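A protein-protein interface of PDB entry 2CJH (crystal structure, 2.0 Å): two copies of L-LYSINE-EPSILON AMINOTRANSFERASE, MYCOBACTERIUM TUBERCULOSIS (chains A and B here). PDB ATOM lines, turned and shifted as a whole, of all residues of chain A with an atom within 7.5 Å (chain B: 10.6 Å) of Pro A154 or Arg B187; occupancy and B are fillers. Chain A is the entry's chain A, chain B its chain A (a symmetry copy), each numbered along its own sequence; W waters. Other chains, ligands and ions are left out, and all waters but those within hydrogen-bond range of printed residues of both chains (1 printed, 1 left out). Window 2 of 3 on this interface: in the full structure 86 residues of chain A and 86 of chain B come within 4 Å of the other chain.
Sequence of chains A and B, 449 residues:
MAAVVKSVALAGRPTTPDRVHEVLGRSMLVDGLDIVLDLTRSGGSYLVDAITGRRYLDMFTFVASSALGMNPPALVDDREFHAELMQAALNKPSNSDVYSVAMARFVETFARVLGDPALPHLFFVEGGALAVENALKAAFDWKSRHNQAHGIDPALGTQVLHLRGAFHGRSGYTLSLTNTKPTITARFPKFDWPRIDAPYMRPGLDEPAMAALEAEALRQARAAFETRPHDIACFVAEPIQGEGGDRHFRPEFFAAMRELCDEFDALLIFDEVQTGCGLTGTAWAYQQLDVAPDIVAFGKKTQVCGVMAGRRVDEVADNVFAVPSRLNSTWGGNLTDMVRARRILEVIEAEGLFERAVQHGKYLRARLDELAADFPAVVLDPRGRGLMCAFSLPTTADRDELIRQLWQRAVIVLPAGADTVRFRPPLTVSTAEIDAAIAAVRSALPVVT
CE1 of Phe B188 touches O of Lys A137, at 3.3 Å. Phe A140 touches Arg B187 (CB to O, 3.6 Å). Phe A140 touches Pro B189. OD1 of Asp A141 touches CD of Arg B187, 3.7 Å away. CG of Arg A145 touches NH1 of Arg B187, at 3.7 Å. O of Thr A158 touches CG of Pro B189, at 3.8 Å. OH of Tyr A173 touches CD2 of Leu B175, at 3.8 Å. Phe B188 touches Tyr A173 (CB to OH, 3.6 Å). Arg B187 touches Arg A326. Phe B188 touches Arg A326.
OD1 of Asp A141 lies within salt-bridge range of NH1 of Arg A145, 3.1 Å away. The side-chain amino group of Lys B190 is in hydrogen-bond range of the backbone carbonyl oxygen of Phe B188, at 2.8 Å. OD2 of Asp A318 is in salt-bridge range of NH2 of Arg A145 (3.3 Å). The side-chain hydroxyl (OG) of Ser A144 lies within hydrogen-bond range of the backbone carbonyl oxygen (O) of Pro A154, 2.6 Å away.
Of the printed residues of chain B, Lys A137 touches Leu B175 and Phe B188. Asp A141 touches one residue of chain B. Of chain B, only Arg B187 (3.7 Å) comes within 4 Å of Arg A145. Of chain B, only Arg B187 (3.9 Å) comes within 4 Å of Pro A154. No residue of chain B comes within 4 Å of Ala A155. Gly A157 touches none of the printed residues of chain B. Of the printed residues of chain B, Tyr A173 touches Leu B175 (3.8 Å), Phe B188 (3.6 Å) and Pro B189 (2.8 Å). Printed residues of chain A within 4 Å of Thr B183: Arg A326 (2.7 Å). Of the printed residues of chain A, Ala B186 touches Arg A326 (2.9 Å). Of the printed residues of chain A, Phe B188 touches Lys A137 (3.3 Å), Tyr A173 (3.6 Å) and Arg A326 (3.4 Å). The nearest residue of chain A that does not touch Arg B187 is Gly A157 (5.2 Å).
Water W1 lies within hydrogen-bond range of O of Ile B184 (2.7 Å), O of Arg A326 (2.7 Å) and NZ of Lys A137 (2.8 Å).
Of the 13 printed residues of chain B, 6 touch a printed residue of chain A. Hydrophobic or aromatic side chains of chain B within 4 Å of the printed part of chain A: Leu B175, Ala B186, Phe B188 and Pro B189. Of the 24 printed residues of chain A, 10 touch a printed residue of chain B. Hydrophobic or aromatic side chains of chain A that line the printed part of chain B: Phe A140, Pro A154 and Tyr A173. Among the printed residues, no Asp or Glu carboxylate lies within 4 Å of a Lys or Arg side-chain nitrogen of the other chain.
The guanidinium group (NH1) of Arg A326 lies within hydrogen-bond range of the backbone carbonyl oxygen (O) of Thr B183 (2.7 Å). The side-chain amide oxygen of Gln A148 lies within hydrogen-bond range of the guanidinium group of Arg B187, 2.8 Å away. The backbone carbonyl oxygen (O) of Pro B189 is in hydrogen-bond range of the side-chain hydroxyl (OH) of Tyr A173 (2.8 Å). NH2 of Arg A326 sits at hydrogen-bond distance from O of Ala B186 (2.9 Å). The guanidinium group of Arg B187 is in hydrogen-bond range of the side-chain hydroxyl of Ser A144 (2.9 Å).
No position is printed for both chains.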
ATOM      1  N   LEU A 136      23.384  -7.780  -3.163  1.00  0.00           N
ATOM      2  CA  LEU A 136      24.140  -9.037  -3.181  1.00  0.00           C
ATOM      3  C   LEU A 136      24.625  -9.432  -4.583  1.00  0.00           C
ATOM      4  O   LEU A 136      25.803  -9.785  -4.757  1.00  0.00           O
ATOM      5  CB  LEU A 136      23.361 -10.198  -2.529  1.00  0.00           C
ATOM      6  CG  LEU A 136      22.853 -10.065  -1.091  1.00  0.00           C
ATOM      7  CD1 LEU A 136      22.162 -11.399  -0.669  1.00  0.00           C
ATOM      8  CD2 LEU A 136      24.009  -9.718  -0.157  1.00  0.00           C
ATOM      9  N   LYS A 137      23.727  -9.418  -5.563  1.00  0.00           N
ATOM     10  CA  LYS A 137      24.119  -9.689  -6.953  1.00  0.00           C
ATOM     11  C   LYS A 137      25.247  -8.757  -7.442  1.00  0.00           C
ATOM     12  O   LYS A 137      26.203  -9.220  -8.084  1.00  0.00           O
ATOM     13  CB  LYS A 137      22.910  -9.620  -7.878  1.00  0.00           C
ATOM     14  CG  LYS A 137      21.864 -10.788  -7.618  1.00  0.00           C
ATOM     15  CD  LYS A 137      20.552 -10.515  -8.357  1.00  0.00           C
ATOM     16  CE  LYS A 137      20.699 -10.766  -9.876  1.00  0.00           C
ATOM     17  NZ  LYS A 137      19.384 -10.492 -10.621  1.00  0.00           N
ATOM     18  N   ALA A 139      27.529  -7.441  -5.631  1.00  0.00           N
ATOM     19  CA  ALA A 139      28.732  -7.860  -4.928  1.00  0.00           C
ATOM     20  C   ALA A 139      29.295  -9.162  -5.480  1.00  0.00           C
ATOM     21  O   ALA A 139      30.523  -9.308  -5.574  1.00  0.00           O
ATOM     22  CB  ALA A 139      28.459  -8.004  -3.401  1.00  0.00           C
ATOM     23  N   PHE A 140      28.430 -10.132  -5.784  1.00  0.00           N
ATOM     24  CA  PHE A 140      28.886 -11.423  -6.317  1.00  0.00           C
ATOM     25  C   PHE A 140      29.591 -11.201  -7.646  1.00  0.00           C
ATOM     26  O   PHE A 140      30.638 -11.806  -7.919  1.00  0.00           O
ATOM     27  CB  PHE A 140      27.717 -12.407  -6.558  1.00  0.00           C
ATOM     28  CG  PHE A 140      26.978 -12.821  -5.296  1.00  0.00           C
ATOM     29  CD1 PHE A 140      27.682 -13.168  -4.149  1.00  0.00           C
ATOM     30  CD2 PHE A 140      25.573 -12.925  -5.285  1.00  0.00           C
ATOM     31  CE1 PHE A 140      27.014 -13.568  -2.975  1.00  0.00           C
ATOM     32  CE2 PHE A 140      24.888 -13.338  -4.099  1.00  0.00           C
ATOM     33  CZ  PHE A 140      25.607 -13.658  -2.962  1.00  0.00           C
ATOM     34  N   ASP A 141      28.998 -10.359  -8.488  1.00  0.00           N
ATOM     35  CA  ASP A 141      29.551 -10.080  -9.800  1.00  0.00           C
ATOM     36  C   ASP A 141      30.894  -9.326  -9.640  1.00  0.00           C
ATOM     37  O   ASP A 141      31.885  -9.609 -10.327  1.00  0.00           O
ATOM     38  CB  ASP A 141      28.561  -9.229 -10.592  1.00  0.00           C
ATOM     39  CG  ASP A 141      29.165  -8.682 -11.885  1.00  0.00           C
ATOM     40  OD1 ASP A 141      29.110  -9.386 -12.936  1.00  0.00           O
ATOM     41  OD2 ASP A 141      29.673  -7.529 -11.835  1.00  0.00           O
ATOM     42  N   TRP A 142      30.895  -8.352  -8.741  1.00  0.00           N
ATOM     43  CA  TRP A 142      32.084  -7.564  -8.481  1.00  0.00           C
ATOM     44  C   TRP A 142      33.242  -8.459  -8.039  1.00  0.00           C
ATOM     45  O   TRP A 142      34.348  -8.348  -8.593  1.00  0.00           O
ATOM     46  CB  TRP A 142      31.794  -6.496  -7.445  1.00  0.00           C
ATOM     47  CG  TRP A 142      32.964  -5.540  -7.188  1.00  0.00           C
ATOM     48  CD1 TRP A 142      33.205  -4.355  -7.811  1.00  0.00           C
ATOM     49  CD2 TRP A 142      34.013  -5.722  -6.236  1.00  0.00           C
ATOM     50  NE1 TRP A 142      34.353  -3.768  -7.304  1.00  0.00           N
ATOM     51  CE2 TRP A 142      34.876  -4.602  -6.349  1.00  0.00           C
ATOM     52  CE3 TRP A 142      34.316  -6.732  -5.303  1.00  0.00           C
ATOM     53  CZ2 TRP A 142      36.013  -4.449  -5.554  1.00  0.00           C
ATOM     54  CZ3 TRP A 142      35.437  -6.577  -4.512  1.00  0.00           C
ATOM     55  CH2 TRP A 142      36.277  -5.440  -4.644  1.00  0.00           C
ATOM     56  N   LYS A 143      32.994  -9.343  -7.069  1.00  0.00           N
ATOM     57  CA  LYS A 143      34.029 -10.233  -6.550  1.00  0.00           C
ATOM     58  C   LYS A 143      34.578 -11.223  -7.603  1.00  0.00           C
ATOM     59  O   LYS A 143      35.794 -11.432  -7.706  1.00  0.00           O
ATOM     60  CB  LYS A 143      33.557 -11.006  -5.324  1.00  0.00           C
ATOM     61  CG  LYS A 143      34.667 -11.813  -4.612  1.00  0.00           C
ATOM     62  CD  LYS A 143      35.722 -10.874  -3.991  1.00  0.00           C
ATOM     63  CE  LYS A 143      36.741 -11.665  -3.187  1.00  0.00           C
ATOM     64  NZ  LYS A 143      37.885 -10.830  -2.700  1.00  0.00           N
ATOM     65  N   SER A 144      33.684 -11.830  -8.367  1.00  0.00           N
ATOM     66  CA  SER A 144      34.079 -12.746  -9.447  1.00  0.00           C
ATOM     67  C   SER A 144      34.997 -11.998 -10.432  1.00  0.00           C
ATOM     68  O   SER A 144      36.079 -12.488 -10.757  1.00  0.00           O
ATOM     69  CB  SER A 144      32.818 -13.252 -10.164  1.00  0.00           C
ATOM     70  OG  SER A 144      33.124 -14.189 -11.184  1.00  0.00           O
ATOM     71  N   ARG A 145      34.570 -10.815 -10.883  1.00  0.00           N
ATOM     72  CA  ARG A 145      35.327 -10.026 -11.869  1.00  0.00           C
ATOM     73  C   ARG A 145      36.646  -9.483 -11.296  1.00  0.00           C
ATOM     74  O   ARG A 145      37.670  -9.498 -11.991  1.00  0.00           O
ATOM     75  CB  ARG A 145      34.469  -8.902 -12.480  1.00  0.00           C
ATOM     76  CG  ARG A 145      33.147  -9.458 -13.009  1.00  0.00           C
ATOM     77  CD  ARG A 145      32.162  -8.433 -13.643  1.00  0.00           C
ATOM     78  NE  ARG A 145      32.397  -8.594 -15.034  1.00  0.00           N
ATOM     79  CZ  ARG A 145      31.559  -8.986 -15.979  1.00  0.00           C
ATOM     80  NH1 ARG A 145      30.266  -9.202 -15.788  1.00  0.00           N
ATOM     81  NH2 ARG A 145      32.078  -9.092 -17.178  1.00  0.00           N
ATOM     82  N   HIS A 146      36.630  -9.066 -10.027  1.00  0.00           N
ATOM     83  CA  HIS A 146      37.840  -8.605  -9.340  1.00  0.00           C
ATOM     84  C   HIS A 146      38.835  -9.777  -9.214  1.00  0.00           C
ATOM     85  O   HIS A 146      40.007  -9.644  -9.573  1.00  0.00           O
ATOM     86  CB  HIS A 146      37.497  -8.035  -7.958  1.00  0.00           C
ATOM     87  CG  HIS A 146      38.643  -7.346  -7.283  1.00  0.00           C
ATOM     88  ND1 HIS A 146      39.504  -7.995  -6.417  1.00  0.00           N
ATOM     89  CD2 HIS A 146      39.075  -6.063  -7.357  1.00  0.00           C
ATOM     90  CE1 HIS A 146      40.408  -7.138  -5.977  1.00  0.00           C
ATOM     91  NE2 HIS A 146      40.177  -5.962  -6.542  1.00  0.00           N
ATOM     92  N   ASN A 147      38.351 -10.919  -8.730  1.00  0.00           N
ATOM     93  CA  ASN A 147      39.114 -12.165  -8.718  1.00  0.00           C
ATOM     94  C   ASN A 147      39.732 -12.475 -10.082  1.00  0.00           C
ATOM     95  O   ASN A 147      40.934 -12.712 -10.167  1.00  0.00           O
ATOM     96  CB  ASN A 147      38.251 -13.343  -8.271  1.00  0.00           C
ATOM     97  CG  ASN A 147      38.112 -13.446  -6.766  1.00  0.00           C
ATOM     98  OD1 ASN A 147      38.869 -12.830  -5.999  1.00  0.00           O
ATOM     99  ND2 ASN A 147      37.153 -14.258  -6.327  1.00  0.00           N
ATOM    100  N   GLN A 148      38.912 -12.480 -11.134  1.00  0.00           N
ATOM    101  CA  GLN A 148      39.364 -12.770 -12.497  1.00  0.00           C
ATOM    102  C   GLN A 148      40.490 -11.813 -12.938  1.00  0.00           C
ATOM    103  O   GLN A 148      41.472 -12.250 -13.554  1.00  0.00           O
ATOM    104  CB  GLN A 148      38.166 -12.702 -13.469  1.00  0.00           C
ATOM    105  CG  GLN A 148      38.480 -13.004 -14.924  1.00  0.00           C
ATOM    106  CD  GLN A 148      37.235 -13.189 -15.821  1.00  0.00           C
ATOM    107  OE1 GLN A 148      36.092 -13.228 -15.363  1.00  0.00           O
ATOM    108  NE2 GLN A 148      37.477 -13.301 -17.117  1.00  0.00           N
ATOM    109  N   ALA A 149      40.354 -10.524 -12.604  1.00  0.00           N
ATOM    110  CA  ALA A 149      41.298  -9.482 -13.044  1.00  0.00           C
ATOM    111  C   ALA A 149      42.633  -9.635 -12.360  1.00  0.00           C
ATOM    112  O   ALA A 149      43.621  -9.077 -12.815  1.00  0.00           O
ATOM    113  CB  ALA A 149      40.744  -8.069 -12.791  1.00  0.00           C
ATOM    114  N   GLY A 151      43.960 -12.772 -11.516  1.00  0.00           N
ATOM    115  CA  GLY A 151      44.410 -14.147 -11.666  1.00  0.00           C
ATOM    116  C   GLY A 151      43.799 -15.180 -10.729  1.00  0.00           C
ATOM    117  O   GLY A 151      44.294 -16.301 -10.642  1.00  0.00           O
ATOM    118  N   ILE A 152      42.723 -14.823 -10.027  1.00  0.00           N
ATOM    119  CA  ILE A 152      41.992 -15.773  -9.173  1.00  0.00           C
ATOM    120  C   ILE A 152      40.801 -16.356  -9.940  1.00  0.00           C
ATOM    121  O   ILE A 152      40.198 -15.679 -10.778  1.00  0.00           O
ATOM    122  CB  ILE A 152      41.578 -15.094  -7.854  1.00  0.00           C
ATOM    123  CG1 ILE A 152      42.839 -14.573  -7.146  1.00  0.00           C
ATOM    124  CG2 ILE A 152      40.815 -16.054  -6.948  1.00  0.00           C
ATOM    125  CD1 ILE A 152      42.619 -13.470  -6.138  1.00  0.00           C
ATOM    126  N   ASP A 153      40.500 -17.625  -9.696  1.00  0.00           N
ATOM    127  CA  ASP A 153      39.368 -18.314 -10.312  1.00  0.00           C
ATOM    128  C   ASP A 153      38.069 -17.463 -10.170  1.00  0.00           C
ATOM    129  O   ASP A 153      37.689 -17.140  -9.034  1.00  0.00           O
ATOM    130  CB  ASP A 153      39.217 -19.666  -9.623  1.00  0.00           C
ATOM    131  CG  ASP A 153      38.106 -20.530 -10.210  1.00  0.00           C
ATOM    132  OD1 ASP A 153      37.527 -20.177 -11.271  1.00  0.00           O
ATOM    133  OD2 ASP A 153      37.801 -21.582  -9.582  1.00  0.00           O
ATOM    134  N   PRO A 154      37.430 -17.073 -11.307  1.00  0.00           N
ATOM    135  CA  PRO A 154      36.142 -16.350 -11.326  1.00  0.00           C
ATOM    136  C   PRO A 154      34.948 -17.131 -10.757  1.00  0.00           C
ATOM    137  O   PRO A 154      33.877 -16.552 -10.543  1.00  0.00           O
ATOM    138  CB  PRO A 154      35.920 -16.044 -12.820  1.00  0.00           C
ATOM    139  CG  PRO A 154      36.735 -17.053 -13.553  1.00  0.00           C
ATOM    140  CD  PRO A 154      37.957 -17.248 -12.683  1.00  0.00           C
ATOM    141  N   ALA A 155      35.123 -18.426 -10.507  1.00  0.00           N
ATOM    142  CA  ALA A 155      34.078 -19.201  -9.864  1.00  0.00           C
ATOM    143  C   ALA A 155      34.028 -18.879  -8.373  1.00  0.00           C
ATOM    144  O   ALA A 155      33.054 -19.226  -7.689  1.00  0.00           O
ATOM    145  CB  ALA A 155      34.288 -20.696 -10.088  1.00  0.00           C
ATOM    146  N   LEU A 156      35.082 -18.239  -7.863  1.00  0.00           N
ATOM    147  CA  LEU A 156      35.135 -17.859  -6.447  1.00  0.00           C
ATOM    148  C   LEU A 156      34.501 -16.469  -6.274  1.00  0.00           C
ATOM    149  O   LEU A 156      34.617 -15.620  -7.181  1.00  0.00           O
ATOM    150  CB  LEU A 156      36.587 -17.860  -5.940  1.00  0.00           C
ATOM    151  CG  LEU A 156      37.294 -19.228  -5.818  1.00  0.00           C
ATOM    152  CD1 LEU A 156      38.764 -19.053  -5.491  1.00  0.00           C
ATOM    153  CD2 LEU A 156      36.624 -20.062  -4.751  1.00  0.00           C
ATOM    154  N   GLY A 157      33.860 -16.257  -5.123  1.00  0.00           N
ATOM    155  CA  GLY A 157      33.191 -14.987  -4.803  1.00  0.00           C
ATOM    156  C   GLY A 157      31.679 -15.137  -4.616  1.00  0.00           C
ATOM    157  O   GLY A 157      30.913 -14.375  -5.178  1.00  0.00           O
ATOM    158  N   THR A 158      31.249 -16.121  -3.825  1.00  0.00           N
ATOM    159  CA  THR A 158      29.840 -16.481  -3.788  1.00  0.00           C
ATOM    160  C   THR A 158      29.222 -16.448  -2.380  1.00  0.00           C
ATOM    161  O   THR A 158      28.060 -16.808  -2.215  1.00  0.00           O
ATOM    162  CB  THR A 158      29.623 -17.908  -4.341  1.00  0.00           C
ATOM    163  OG1 THR A 158      30.400 -18.826  -3.565  1.00  0.00           O
ATOM    164  CG2 THR A 158      30.046 -18.012  -5.842  1.00  0.00           C
ATOM    165  N   TYR A 173      17.710 -15.513  -1.661  1.00  0.00           N
ATOM    166  CA  TYR A 173      19.015 -15.237  -1.014  1.00  0.00           C
ATOM    167  C   TYR A 173      18.907 -14.762   0.434  1.00  0.00           C
ATOM    168  O   TYR A 173      19.748 -15.111   1.278  1.00  0.00           O
ATOM    169  CB  TYR A 173      19.838 -14.190  -1.790  1.00  0.00           C
ATOM    170  CG  TYR A 173      20.456 -14.647  -3.091  1.00  0.00           C
ATOM    171  CD1 TYR A 173      20.875 -15.967  -3.274  1.00  0.00           C
ATOM    172  CD2 TYR A 173      20.610 -13.752  -4.156  1.00  0.00           C
ATOM    173  CE1 TYR A 173      21.458 -16.380  -4.480  1.00  0.00           C
ATOM    174  CE2 TYR A 173      21.193 -14.156  -5.372  1.00  0.00           C
ATOM    175  CZ  TYR A 173      21.616 -15.466  -5.515  1.00  0.00           C
ATOM    176  OH  TYR A 173      22.190 -15.862  -6.699  1.00  0.00           O
ATOM    177  N   ASP A 318      33.342  -3.189 -15.581  1.00  0.00           N
ATOM    178  CA  ASP A 318      32.207  -3.913 -16.182  1.00  0.00           C
ATOM    179  C   ASP A 318      31.297  -4.494 -15.083  1.00  0.00           C
ATOM    180  O   ASP A 318      30.820  -5.603 -15.189  1.00  0.00           O
ATOM    181  CB  ASP A 318      32.669  -4.972 -17.206  1.00  0.00           C
ATOM    182  CG  ASP A 318      33.879  -5.801 -16.724  1.00  0.00           C
ATOM    183  OD1 ASP A 318      34.429  -5.535 -15.638  1.00  0.00           O
ATOM    184  OD2 ASP A 318      34.309  -6.721 -17.450  1.00  0.00           O
ATOM    185  N   ARG A 326      22.237  -7.067 -16.626  1.00  0.00           N
ATOM    186  CA  ARG A 326      22.707  -7.899 -15.503  1.00  0.00           C
ATOM    187  C   ARG A 326      21.721  -7.840 -14.325  1.00  0.00           C
ATOM    188  O   ARG A 326      21.531  -8.849 -13.633  1.00  0.00           O
ATOM    189  CB  ARG A 326      24.115  -7.477 -15.038  1.00  0.00           C
ATOM    190  CG  ARG A 326      25.199  -7.659 -16.108  1.00  0.00           C
ATOM    191  CD  ARG A 326      25.548  -9.096 -16.243  1.00  0.00           C
ATOM    192  NE  ARG A 326      26.313  -9.567 -15.102  1.00  0.00           N
ATOM    193  CZ  ARG A 326      26.202 -10.779 -14.565  1.00  0.00           C
ATOM    194  NH1 ARG A 326      25.316 -11.660 -15.051  1.00  0.00           N
ATOM    195  NH2 ARG A 326      26.967 -11.113 -13.534  1.00  0.00           N
ATOM    196  N   LEU B 175      16.922 -17.556  -9.979  1.00  0.00           N
ATOM    197  CA  LEU B 175      18.189 -17.580 -10.708  1.00  0.00           C
ATOM    198  C   LEU B 175      18.723 -18.992 -10.857  1.00  0.00           C
ATOM    199  O   LEU B 175      19.539 -19.259 -11.733  1.00  0.00           O
ATOM    200  CB  LEU B 175      19.235 -16.712 -10.000  1.00  0.00           C
ATOM    201  CG  LEU B 175      19.673 -15.296 -10.411  1.00  0.00           C
ATOM    202  CD1 LEU B 175      19.061 -14.653 -11.678  1.00  0.00           C
ATOM    203  CD2 LEU B 175      19.728 -14.377  -9.185  1.00  0.00           C
ATOM    204  N   SER B 176      18.259 -19.913 -10.002  1.00  0.00           N
ATOM    205  CA  SER B 176      18.598 -21.349 -10.181  1.00  0.00           C
ATOM    206  C   SER B 176      17.690 -22.065 -11.175  1.00  0.00           C
ATOM    207  O   SER B 176      17.929 -23.244 -11.518  1.00  0.00           O
ATOM    208  CB  SER B 176      18.567 -22.075  -8.849  1.00  0.00           C
ATOM    209  OG  SER B 176      19.525 -21.516  -7.966  1.00  0.00           O
ATOM    210  N   THR B 178      15.848 -20.086 -14.011  1.00  0.00           N
ATOM    211  CA  THR B 178      16.000 -19.342 -15.273  1.00  0.00           C
ATOM    212  C   THR B 178      17.268 -19.761 -16.027  1.00  0.00           C
ATOM    213  O   THR B 178      18.356 -19.796 -15.464  1.00  0.00           O
ATOM    214  CB  THR B 178      16.042 -17.808 -15.010  1.00  0.00           C
ATOM    215  OG1 THR B 178      14.823 -17.422 -14.379  1.00  0.00           O
ATOM    216  CG2 THR B 178      16.187 -17.012 -16.319  1.00  0.00           C
ATOM    217  N   LYS B 181      19.375 -16.430 -21.552  1.00  0.00           N
ATOM    218  CA  LYS B 181      20.621 -15.697 -21.818  1.00  0.00           C
ATOM    219  C   LYS B 181      21.564 -15.816 -20.615  1.00  0.00           C
ATOM    220  O   LYS B 181      21.153 -15.541 -19.471  1.00  0.00           O
ATOM    221  CB  LYS B 181      20.344 -14.197 -22.031  1.00  0.00           C
ATOM    222  CG  LYS B 181      19.376 -13.824 -23.151  1.00  0.00           C
ATOM    223  CD  LYS B 181      20.034 -13.931 -24.535  1.00  0.00           C
ATOM    224  CE  LYS B 181      19.581 -12.767 -25.457  1.00  0.00           C
ATOM    225  NZ  LYS B 181      18.151 -12.376 -25.207  1.00  0.00           N
ATOM    226  N   PRO B 182      22.840 -16.180 -20.856  1.00  0.00           N
ATOM    227  CA  PRO B 182      23.872 -16.265 -19.798  1.00  0.00           C
ATOM    228  C   PRO B 182      24.026 -14.980 -18.995  1.00  0.00           C
ATOM    229  O   PRO B 182      24.349 -15.032 -17.817  1.00  0.00           O
ATOM    230  CB  PRO B 182      25.158 -16.540 -20.593  1.00  0.00           C
ATOM    231  CG  PRO B 182      24.676 -17.299 -21.793  1.00  0.00           C
ATOM    232  CD  PRO B 182      23.390 -16.555 -22.169  1.00  0.00           C
ATOM    233  N   THR B 183      23.803 -13.837 -19.644  1.00  0.00           N
ATOM    234  CA  THR B 183      23.829 -12.533 -18.991  1.00  0.00           C
ATOM    235  C   THR B 183      22.928 -12.451 -17.734  1.00  0.00           C
ATOM    236  O   THR B 183      23.243 -11.725 -16.782  1.00  0.00           O
ATOM    237  CB  THR B 183      23.410 -11.446 -20.020  1.00  0.00           C
ATOM    238  OG1 THR B 183      24.383 -11.443 -21.064  1.00  0.00           O
ATOM    239  CG2 THR B 183      23.336 -10.036 -19.412  1.00  0.00           C
ATOM    240  N   ILE B 184      21.806 -13.167 -17.738  1.00  0.00           N
ATOM    241  CA  ILE B 184      20.871 -13.111 -16.600  1.00  0.00           C
ATOM    242  C   ILE B 184      21.430 -13.784 -15.335  1.00  0.00           C
ATOM    243  O   ILE B 184      21.214 -13.288 -14.212  1.00  0.00           O
ATOM    244  CB  ILE B 184      19.492 -13.704 -16.983  1.00  0.00           C
ATOM    245  CG1 ILE B 184      18.935 -12.947 -18.198  1.00  0.00           C
ATOM    246  CG2 ILE B 184      18.516 -13.665 -15.798  1.00  0.00           C
ATOM    247  CD1 ILE B 184      17.669 -13.616 -18.820  1.00  0.00           C
ATOM    248  N   THR B 185      22.189 -14.862 -15.534  1.00  0.00           N
ATOM    249  CA  THR B 185      22.521 -15.803 -14.465  1.00  0.00           C
ATOM    250  C   THR B 185      24.012 -15.882 -14.130  1.00  0.00           C
ATOM    251  O   THR B 185      24.364 -16.350 -13.069  1.00  0.00           O
ATOM    252  CB  THR B 185      21.976 -17.251 -14.768  1.00  0.00           C
ATOM    253  OG1 THR B 185      22.305 -17.618 -16.115  1.00  0.00           O
ATOM    254  CG2 THR B 185      20.446 -17.283 -14.635  1.00  0.00           C
ATOM    255  N   ALA B 186      24.877 -15.406 -15.026  1.00  0.00           N
ATOM    256  CA  ALA B 186      26.328 -15.643 -14.891  1.00  0.00           C
ATOM    257  C   ALA B 186      26.879 -15.027 -13.589  1.00  0.00           C
ATOM    258  O   ALA B 186      26.477 -13.933 -13.213  1.00  0.00           O
ATOM    259  CB  ALA B 186      27.068 -15.089 -16.126  1.00  0.00           C
ATOM    260  N   ARG B 187      27.770 -15.745 -12.907  1.00  0.00           N
ATOM    261  CA  ARG B 187      28.441 -15.248 -11.689  1.00  0.00           C
ATOM    262  C   ARG B 187      27.545 -15.093 -10.433  1.00  0.00           C
ATOM    263  O   ARG B 187      27.989 -14.513  -9.437  1.00  0.00           O
ATOM    264  CB  ARG B 187      29.198 -13.920 -11.955  1.00  0.00           C
ATOM    265  CG  ARG B 187      30.115 -13.936 -13.198  1.00  0.00           C
ATOM    266  CD  ARG B 187      30.876 -12.611 -13.393  1.00  0.00           C
ATOM    267  NE  ARG B 187      31.588 -12.634 -14.681  1.00  0.00           N
ATOM    268  CZ  ARG B 187      32.900 -12.835 -14.833  1.00  0.00           C
ATOM    269  NH1 ARG B 187      33.710 -13.002 -13.784  1.00  0.00           N
ATOM    270  NH2 ARG B 187      33.409 -12.831 -16.060  1.00  0.00           N
ATOM    271  N   PHE B 188      26.309 -15.601 -10.475  1.00  0.00           N
ATOM    272  CA  PHE B 188      25.396 -15.563  -9.299  1.00  0.00           C
ATOM    273  C   PHE B 188      25.297 -16.988  -8.709  1.00  0.00           C
ATOM    274  O   PHE B 188      25.176 -17.954  -9.464  1.00  0.00           O
ATOM    275  CB  PHE B 188      24.029 -15.003  -9.732  1.00  0.00           C
ATOM    276  CG  PHE B 188      24.095 -13.607 -10.342  1.00  0.00           C
ATOM    277  CD1 PHE B 188      24.870 -12.580  -9.738  1.00  0.00           C
ATOM    278  CD2 PHE B 188      23.400 -13.312 -11.508  1.00  0.00           C
ATOM    279  CE1 PHE B 188      24.942 -11.311 -10.312  1.00  0.00           C
ATOM    280  CE2 PHE B 188      23.448 -12.036 -12.078  1.00  0.00           C
ATOM    281  CZ  PHE B 188      24.215 -11.028 -11.473  1.00  0.00           C
ATOM    282  N   PRO B 189      25.446 -17.151  -7.388  1.00  0.00           N
ATOM    283  CA  PRO B 189      25.345 -18.517  -6.867  1.00  0.00           C
ATOM    284  C   PRO B 189      23.976 -19.201  -7.069  1.00  0.00           C
ATOM    285  O   PRO B 189      22.923 -18.544  -7.052  1.00  0.00           O
ATOM    286  CB  PRO B 189      25.674 -18.386  -5.375  1.00  0.00           C
ATOM    287  CG  PRO B 189      25.558 -16.893  -5.054  1.00  0.00           C
ATOM    288  CD  PRO B 189      25.804 -16.164  -6.346  1.00  0.00           C
ATOM    289  N   LYS B 190      24.035 -20.508  -7.279  1.00  0.00           N
ATOM    290  CA  LYS B 190      22.855 -21.293  -7.659  1.00  0.00           C
ATOM    291  C   LYS B 190      22.791 -22.605  -6.884  1.00  0.00           C
ATOM    292  O   LYS B 190      23.801 -23.090  -6.382  1.00  0.00           O
ATOM    293  CB  LYS B 190      22.824 -21.544  -9.170  1.00  0.00           C
ATOM    294  CG  LYS B 190      22.771 -20.270  -9.986  1.00  0.00           C
ATOM    295  CD  LYS B 190      22.793 -20.515 -11.501  1.00  0.00           C
ATOM    296  CE  LYS B 190      24.168 -20.304 -12.106  1.00  0.00           C
ATOM    297  NZ  LYS B 190      24.702 -18.880 -12.050  1.00  0.00           N
HETATM  298  O   HOH W   1      19.984 -11.083 -13.333  1.00  0.00           O
